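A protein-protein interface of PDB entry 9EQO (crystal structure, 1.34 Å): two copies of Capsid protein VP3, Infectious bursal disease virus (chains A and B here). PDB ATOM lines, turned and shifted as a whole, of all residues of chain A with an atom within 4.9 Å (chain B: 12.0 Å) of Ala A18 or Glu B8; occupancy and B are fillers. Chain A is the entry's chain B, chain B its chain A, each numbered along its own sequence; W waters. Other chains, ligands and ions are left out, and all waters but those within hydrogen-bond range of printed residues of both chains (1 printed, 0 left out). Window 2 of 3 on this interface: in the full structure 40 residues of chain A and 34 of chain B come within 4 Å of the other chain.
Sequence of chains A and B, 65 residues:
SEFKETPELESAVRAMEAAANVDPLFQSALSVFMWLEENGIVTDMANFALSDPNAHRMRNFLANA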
ATOM      1  N   ARG A  14     -10.870  33.874  22.950  1.00  0.00           N
ATOM      2  CA  ARG A  14     -10.337  32.638  23.507  1.00  0.00           C
ATOM      3  C   ARG A  14      -9.902  31.683  22.404  1.00  0.00           C
ATOM      4  O   ARG A  14      -8.832  31.068  22.487  1.00  0.00           O
ATOM      5  CB  ARG A  14     -11.406  31.985  24.381  1.00  0.00           C
ATOM      6  CG  ARG A  14     -10.939  30.718  25.081  1.00  0.00           C
ATOM      7  CD  ARG A  14     -12.102  29.817  25.496  1.00  0.00           C
ATOM      8  NE  ARG A  14     -13.045  30.464  26.400  1.00  0.00           N
ATOM      9  CZ  ARG A  14     -14.329  30.678  26.130  1.00  0.00           C
ATOM     10  NH1 ARG A  14     -14.861  30.324  24.970  1.00  0.00           N
ATOM     11  NH2 ARG A  14     -15.101  31.248  27.052  1.00  0.00           N
ATOM     12  N   ALA A  15     -10.715  31.551  21.356  1.00  0.00           N
ATOM     13  CA  ALA A  15     -10.375  30.659  20.253  1.00  0.00           C
ATOM     14  C   ALA A  15      -9.139  31.151  19.510  1.00  0.00           C
ATOM     15  O   ALA A  15      -8.274  30.353  19.131  1.00  0.00           O
ATOM     16  CB  ALA A  15     -11.556  30.532  19.295  1.00  0.00           C
ATOM     17  N   MET A  16      -9.027  32.462  19.308  1.00  0.00           N
ATOM     18  CA  MET A  16      -7.850  32.998  18.634  1.00  0.00           C
ATOM     19  C   MET A  16      -6.598  32.785  19.473  1.00  0.00           C
ATOM     20  O   MET A  16      -5.526  32.492  18.928  1.00  0.00           O
ATOM     21  CB  MET A  16      -8.055  34.478  18.329  1.00  0.00           C
ATOM     22  CG  MET A  16      -9.114  34.761  17.271  1.00  0.00           C
ATOM     23  SD  MET A  16      -9.400  36.525  17.003  1.00  0.00           S
ATOM     24  CE  MET A  16      -7.934  36.918  16.053  1.00  0.00           C
ATOM     25  N   GLU A  17      -6.718  32.921  20.796  1.00  0.00           N
ATOM     26  CA  GLU A  17      -5.596  32.640  21.687  1.00  0.00           C
ATOM     27  C   GLU A  17      -5.183  31.174  21.625  1.00  0.00           C
ATOM     28  O   GLU A  17      -3.985  30.867  21.607  1.00  0.00           O
ATOM     29  CB  GLU A  17      -5.939  33.072  23.113  1.00  0.00           C
ATOM     30  CG  GLU A  17      -5.994  34.597  23.269  1.00  0.00           C
ATOM     31  CD  GLU A  17      -6.554  35.059  24.602  1.00  0.00           C
ATOM     32  OE1 GLU A  17      -7.192  34.244  25.305  1.00  0.00           O
ATOM     33  OE2 GLU A  17      -6.356  36.246  24.940  1.00  0.00           O
ATOM     34  N   ALA A  18      -6.148  30.255  21.536  1.00  0.00           N
ATOM     35  CA  ALA A  18      -5.812  28.839  21.399  1.00  0.00           C
ATOM     36  C   ALA A  18      -5.092  28.567  20.079  1.00  0.00           C
ATOM     37  O   ALA A  18      -4.159  27.760  20.025  1.00  0.00           O
ATOM     38  CB  ALA A  18      -7.070  27.976  21.535  1.00  0.00           C
ATOM     39  N   ALA A  19      -5.494  29.252  19.007  1.00  0.00           N
ATOM     40  CA  ALA A  19      -4.819  29.088  17.727  1.00  0.00           C
ATOM     41  C   ALA A  19      -3.445  29.744  17.737  1.00  0.00           C
ATOM     42  O   ALA A  19      -2.499  29.225  17.131  1.00  0.00           O
ATOM     43  CB  ALA A  19      -5.692  29.666  16.615  1.00  0.00           C
ATOM     44  N   ALA A  20      -3.299  30.859  18.453  1.00  0.00           N
ATOM     45  CA  ALA A  20      -2.004  31.520  18.540  1.00  0.00           C
ATOM     46  C   ALA A  20      -0.977  30.659  19.261  1.00  0.00           C
ATOM     47  O   ALA A  20       0.234  30.858  19.078  1.00  0.00           O
ATOM     48  CB  ALA A  20      -2.174  32.865  19.240  1.00  0.00           C
ATOM     49  N   ASN A  21      -1.434  29.695  20.053  1.00  0.00           N
ATOM     50  CA  ASN A  21      -0.574  28.751  20.745  1.00  0.00           C
ATOM     51  C   ASN A  21       0.051  27.725  19.801  1.00  0.00           C
ATOM     52  O   ASN A  21       1.005  27.047  20.203  1.00  0.00           O
ATOM     53  CB  ASN A  21      -1.433  28.046  21.799  1.00  0.00           C
ATOM     54  CG  ASN A  21      -0.624  27.406  22.907  1.00  0.00           C
ATOM     55  OD1 ASN A  21       0.302  28.010  23.454  1.00  0.00           O
ATOM     56  ND2 ASN A  21      -0.990  26.181  23.262  1.00  0.00           N
ATOM     57  N   VAL A  22      -0.455  27.588  18.571  1.00  0.00           N
ATOM     58  CA  VAL A  22       0.061  26.592  17.632  1.00  0.00           C
ATOM     59  C   VAL A  22       0.457  27.190  16.283  1.00  0.00           C
ATOM     60  O   VAL A  22       1.105  26.516  15.476  1.00  0.00           O
ATOM     61  CB  VAL A  22      -0.927  25.423  17.437  1.00  0.00           C
ATOM     62  CG1 VAL A  22      -1.320  24.803  18.776  1.00  0.00           C
ATOM     63  CG2 VAL A  22      -2.157  25.886  16.673  1.00  0.00           C
ATOM     64  N   GLU B   5      -5.598  23.302   8.860  1.00  0.00           N
ATOM     65  CA  GLU B   5      -6.147  21.934   9.058  1.00  0.00           C
ATOM     66  C   GLU B   5      -5.947  21.504  10.517  1.00  0.00           C
ATOM     67  O   GLU B   5      -6.691  20.612  10.968  1.00  0.00           O
ATOM     68  CB  GLU B   5      -5.493  20.938   8.097  1.00  0.00           C
ATOM     69  CG  GLU B   5      -3.999  20.770   8.310  1.00  0.00           C
ATOM     70  CD  GLU B   5      -3.309  19.878   7.293  1.00  0.00           C
ATOM     71  OE1 GLU B   5      -4.013  19.107   6.613  1.00  0.00           O
ATOM     72  OE2 GLU B   5      -2.071  19.965   7.176  1.00  0.00           O
ATOM     73  N   THR B   6      -5.308  22.614  11.240  1.00  0.00           N
ATOM     74  CA  THR B   6      -5.242  22.243  12.669  1.00  0.00           C
ATOM     75  C   THR B   6      -6.642  22.473  13.223  1.00  0.00           C
ATOM     76  O   THR B   6      -7.335  23.379  12.751  1.00  0.00           O
ATOM     77  CB  THR B   6      -4.241  23.056  13.490  1.00  0.00           C
ATOM     78  OG1 THR B   6      -4.611  24.435  13.423  1.00  0.00           O
ATOM     79  CG2 THR B   6      -2.814  22.854  13.035  1.00  0.00           C
ATOM     80  N   PRO B   7      -7.100  21.650  14.163  1.00  0.00           N
ATOM     81  CA  PRO B   7      -8.395  21.921  14.808  1.00  0.00           C
ATOM     82  C   PRO B   7      -8.473  23.307  15.420  1.00  0.00           C
ATOM     83  O   PRO B   7      -9.555  23.905  15.430  1.00  0.00           O
ATOM     84  CB  PRO B   7      -8.513  20.810  15.866  1.00  0.00           C
ATOM     85  CG  PRO B   7      -7.143  20.238  16.009  1.00  0.00           C
ATOM     86  CD  PRO B   7      -6.459  20.433  14.690  1.00  0.00           C
ATOM     87  N   GLU B   8      -7.352  23.848  15.906  1.00  0.00           N
ATOM     88  CA  GLU B   8      -7.378  25.181  16.504  1.00  0.00           C
ATOM     89  C   GLU B   8      -7.711  26.247  15.467  1.00  0.00           C
ATOM     90  O   GLU B   8      -8.483  27.173  15.744  1.00  0.00           O
ATOM     91  CB  GLU B   8      -6.040  25.483  17.179  1.00  0.00           C
ATOM     92  CG  GLU B   8      -5.754  24.645  18.420  1.00  0.00           C
ATOM     93  CD  GLU B   8      -5.243  23.247  18.101  1.00  0.00           C
ATOM     94  OE1 GLU B   8      -4.940  22.961  16.923  1.00  0.00           O
ATOM     95  OE2 GLU B   8      -5.147  22.425  19.038  1.00  0.00           O
ATOM     96  N   LEU B   9      -7.143  26.131  14.266  1.00  0.00           N
ATOM     97  CA  LEU B   9      -7.430  27.105  13.218  1.00  0.00           C
ATOM     98  C   LEU B   9      -8.895  27.047  12.810  1.00  0.00           C
ATOM     99  O   LEU B   9      -9.574  28.081  12.747  1.00  0.00           O
ATOM    100  CB  LEU B   9      -6.511  26.868  12.017  1.00  0.00           C
ATOM    101  CG  LEU B   9      -6.629  27.873  10.868  1.00  0.00           C
ATOM    102  CD1 LEU B   9      -5.272  28.064  10.195  1.00  0.00           C
ATOM    103  CD2 LEU B   9      -7.677  27.441   9.840  1.00  0.00           C
ATOM    104  N   GLU B  10      -9.403  25.848  12.521  1.00  0.00           N
ATOM    105  CA  GLU B  10     -10.791  25.729  12.089  1.00  0.00           C
ATOM    106  C   GLU B  10     -11.749  26.230  13.159  1.00  0.00           C
ATOM    107  O   GLU B  10     -12.733  26.912  12.854  1.00  0.00           O
ATOM    108  CB  GLU B  10     -11.102  24.286  11.692  1.00  0.00           C
ATOM    109  CG  GLU B  10     -10.231  23.790  10.546  1.00  0.00           C
ATOM    110  CD  GLU B  10     -10.784  22.554   9.866  1.00  0.00           C
ATOM    111  OE1 GLU B  10     -11.495  21.767  10.532  1.00  0.00           O
ATOM    112  OE2 GLU B  10     -10.507  22.374   8.660  1.00  0.00           O
ATOM    113  N   SER B  11     -11.462  25.932  14.427  1.00  0.00           N
ATOM    114  CA  SER B  11     -12.331  26.389  15.501  1.00  0.00           C
ATOM    115  C   SER B  11     -12.279  27.904  15.646  1.00  0.00           C
ATOM    116  O   SER B  11     -13.309  28.545  15.883  1.00  0.00           O
ATOM    117  CB  SER B  11     -11.931  25.706  16.807  1.00  0.00           C
ATOM    118  OG  SER B  11     -12.874  25.974  17.826  1.00  0.00           O
ATOM    119  N   ALA B  12     -11.091  28.494  15.493  1.00  0.00           N
ATOM    120  CA  ALA B  12     -10.965  29.942  15.609  1.00  0.00           C
ATOM    121  C   ALA B  12     -11.734  30.652  14.505  1.00  0.00           C
ATOM    122  O   ALA B  12     -12.376  31.675  14.753  1.00  0.00           O
ATOM    123  CB  ALA B  12      -9.496  30.357  15.598  1.00  0.00           C
ATOM    124  N   VAL B  13     -11.676  30.133  13.277  1.00  0.00           N
ATOM    125  CA  VAL B  13     -12.418  30.771  12.195  1.00  0.00           C
ATOM    126  C   VAL B  13     -13.919  30.699  12.456  1.00  0.00           C
ATOM    127  O   VAL B  13     -14.635  31.685  12.268  1.00  0.00           O
ATOM    128  CB  VAL B  13     -12.013  30.189  10.829  1.00  0.00           C
ATOM    129  CG1 VAL B  13     -12.893  30.767   9.733  1.00  0.00           C
ATOM    130  CG2 VAL B  13     -10.547  30.500  10.536  1.00  0.00           C
ATOM    131  N   ARG B  14     -14.414  29.543  12.918  1.00  0.00           N
ATOM    132  CA  ARG B  14     -15.830  29.441  13.263  1.00  0.00           C
ATOM    133  C   ARG B  14     -16.209  30.435  14.352  1.00  0.00           C
ATOM    134  O   ARG B  14     -17.241  31.110  14.253  1.00  0.00           O
ATOM    135  CB  ARG B  14     -16.176  28.010  13.689  1.00  0.00           C
ATOM    136  CG  ARG B  14     -16.183  26.991  12.552  1.00  0.00           C
ATOM    137  CD  ARG B  14     -16.808  25.657  12.982  1.00  0.00           C
ATOM    138  NE  ARG B  14     -16.086  25.012  14.076  1.00  0.00           N
ATOM    139  CZ  ARG B  14     -15.090  24.145  13.922  1.00  0.00           C
ATOM    140  NH1 ARG B  14     -14.655  23.798  12.721  1.00  0.00           N
ATOM    141  NH2 ARG B  14     -14.518  23.614  15.000  1.00  0.00           N
ATOM    142  N   ALA B  15     -15.380  30.554  15.392  1.00  0.00           N
ATOM    143  CA  ALA B  15     -15.698  31.469  16.482  1.00  0.00           C
ATOM    144  C   ALA B  15     -15.645  32.919  16.019  1.00  0.00           C
ATOM    145  O   ALA B  15     -16.475  33.736  16.432  1.00  0.00           O
ATOM    146  CB  ALA B  15     -14.752  31.238  17.659  1.00  0.00           C
ATOM    147  N   MET B  16     -14.677  33.256  15.161  1.00  0.00           N
ATOM    148  CA  MET B  16     -14.603  34.619  14.649  1.00  0.00           C
ATOM    149  C   MET B  16     -15.816  34.946  13.795  1.00  0.00           C
ATOM    150  O   MET B  16     -16.349  36.057  13.867  1.00  0.00           O
ATOM    151  CB  MET B  16     -13.315  34.813  13.852  1.00  0.00           C
ATOM    152  CG  MET B  16     -12.049  34.836  14.699  1.00  0.00           C
ATOM    153  SD  MET B  16     -10.557  34.794  13.694  1.00  0.00           S
ATOM    154  CE  MET B  16     -10.502  36.464  13.091  1.00  0.00           C
ATOM    155  N   GLU B  17     -16.278  33.986  12.988  1.00  0.00           N
ATOM    156  CA  GLU B  17     -17.477  34.215  12.189  1.00  0.00           C
ATOM    157  C   GLU B  17     -18.699  34.439  13.067  1.00  0.00           C
ATOM    158  O   GLU B  17     -19.533  35.303  12.770  1.00  0.00           O
ATOM    159  CB  GLU B  17     -17.689  33.056  11.215  1.00  0.00           C
ATOM    160  CG  GLU B  17     -16.713  33.119  10.048  1.00  0.00           C
ATOM    161  CD  GLU B  17     -16.657  31.848   9.226  1.00  0.00           C
ATOM    162  OE1 GLU B  17     -17.120  30.794   9.707  1.00  0.00           O
ATOM    163  OE2 GLU B  17     -16.125  31.909   8.092  1.00  0.00           O
ATOM    164  N   LEU B  30     -12.798  40.962  10.755  1.00  0.00           N
ATOM    165  CA  LEU B  30     -12.649  39.640  10.162  1.00  0.00           C
ATOM    166  C   LEU B  30     -12.383  39.742   8.666  1.00  0.00           C
ATOM    167  O   LEU B  30     -11.552  39.003   8.121  1.00  0.00           O
ATOM    168  CB  LEU B  30     -13.891  38.795  10.442  1.00  0.00           C
ATOM    169  CG  LEU B  30     -13.915  37.405   9.802  1.00  0.00           C
ATOM    170  CD1 LEU B  30     -12.719  36.578  10.230  1.00  0.00           C
ATOM    171  CD2 LEU B  30     -15.212  36.700  10.177  1.00  0.00           C
ATOM    172  N   PHE B  33      -8.834  40.544   8.301  1.00  0.00           N
ATOM    173  CA  PHE B  33      -8.041  39.348   8.564  1.00  0.00           C
ATOM    174  C   PHE B  33      -8.017  38.428   7.350  1.00  0.00           C
ATOM    175  O   PHE B  33      -6.953  37.946   6.947  1.00  0.00           O
ATOM    176  CB  PHE B  33      -8.565  38.601   9.793  1.00  0.00           C
ATOM    177  CG  PHE B  33      -7.917  37.261   9.977  1.00  0.00           C
ATOM    178  CD1 PHE B  33      -6.592  37.172  10.386  1.00  0.00           C
ATOM    179  CD2 PHE B  33      -8.601  36.093   9.672  1.00  0.00           C
ATOM    180  CE1 PHE B  33      -5.976  35.939  10.527  1.00  0.00           C
ATOM    181  CE2 PHE B  33      -7.993  34.852   9.819  1.00  0.00           C
ATOM    182  CZ  PHE B  33      -6.680  34.778  10.248  1.00  0.00           C
HETATM  183  O   HOH W   1      -9.005  27.726  18.434  1.00  0.00           O
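Ala A15 touches Ala B12. CB of Ala B15 touches CB of Ala A15, at 3.7 Å. Met A16 touches Met B16. Ala A18 touches Glu B8 (O to CG, 3.9 Å). Ala A19 touches Glu B8. CB of Ala A19 touches CB of Ala B12, at 3.998 Å. CG2 of Val A22 touches CB of Glu B8 (3.9 Å).
Printed residues of chain B within 4 Å of Met A16: Met B16. Ala A18 touches just one residue of chain B: Glu B8. No residue of chain B comes within 4 Å of Ala A20. No residue of chain B comes within 4 Å of Asn A21. Glu B8 touches three residues of chain A. Leu B9 touches none of the printed residues of chain A. Glu B10 touches none of the printed residues of chain A. Of the printed residues of chain A, Ala B12 touches Ala A15 (3.7 Å) and Ala A19 (3.998 Å). Of the printed residues of chain A, Met B16 touches Met A16 (3.9 Å). The nearest residue of chain A that does not touch Glu B8 is Ala A15 (4.7 Å).
Of the 15 printed residues of chain B, 4 touch a printed residue of chain A. Hydrophobic or aromatic side chains of chain B that line the printed part of chain A: Ala B12, Ala B15 and Met B16. Printed residues of chain A that touch a printed residue of chain B: Ala A15, Met A16, Ala A18, Ala A19 and Val A22. Hydrophobic or aromatic side chains of chain A within 4 Å of the printed part of chain B: Ala A15, Met A16, Ala A19 and Val A22. Among the printed residues, 7 pairs touch across the chains. Among the printed residues, no Asp or Glu carboxylate lies within 4 Å of a Lys or Arg side-chain nitrogen of the other chain.
Ala B15 touches its own counterpart, Ala A15. Met A16 touches its own counterpart, Met B16. 4 positions are printed for both chains. Of the 7 pairs that touch across the chains among the printed residues, 2 have their exchanged pair printed and touching as well.
Water W1 bridges the backbone carbonyl oxygen of Glu B8 and the backbone carbonyl oxygen of Ala A15.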
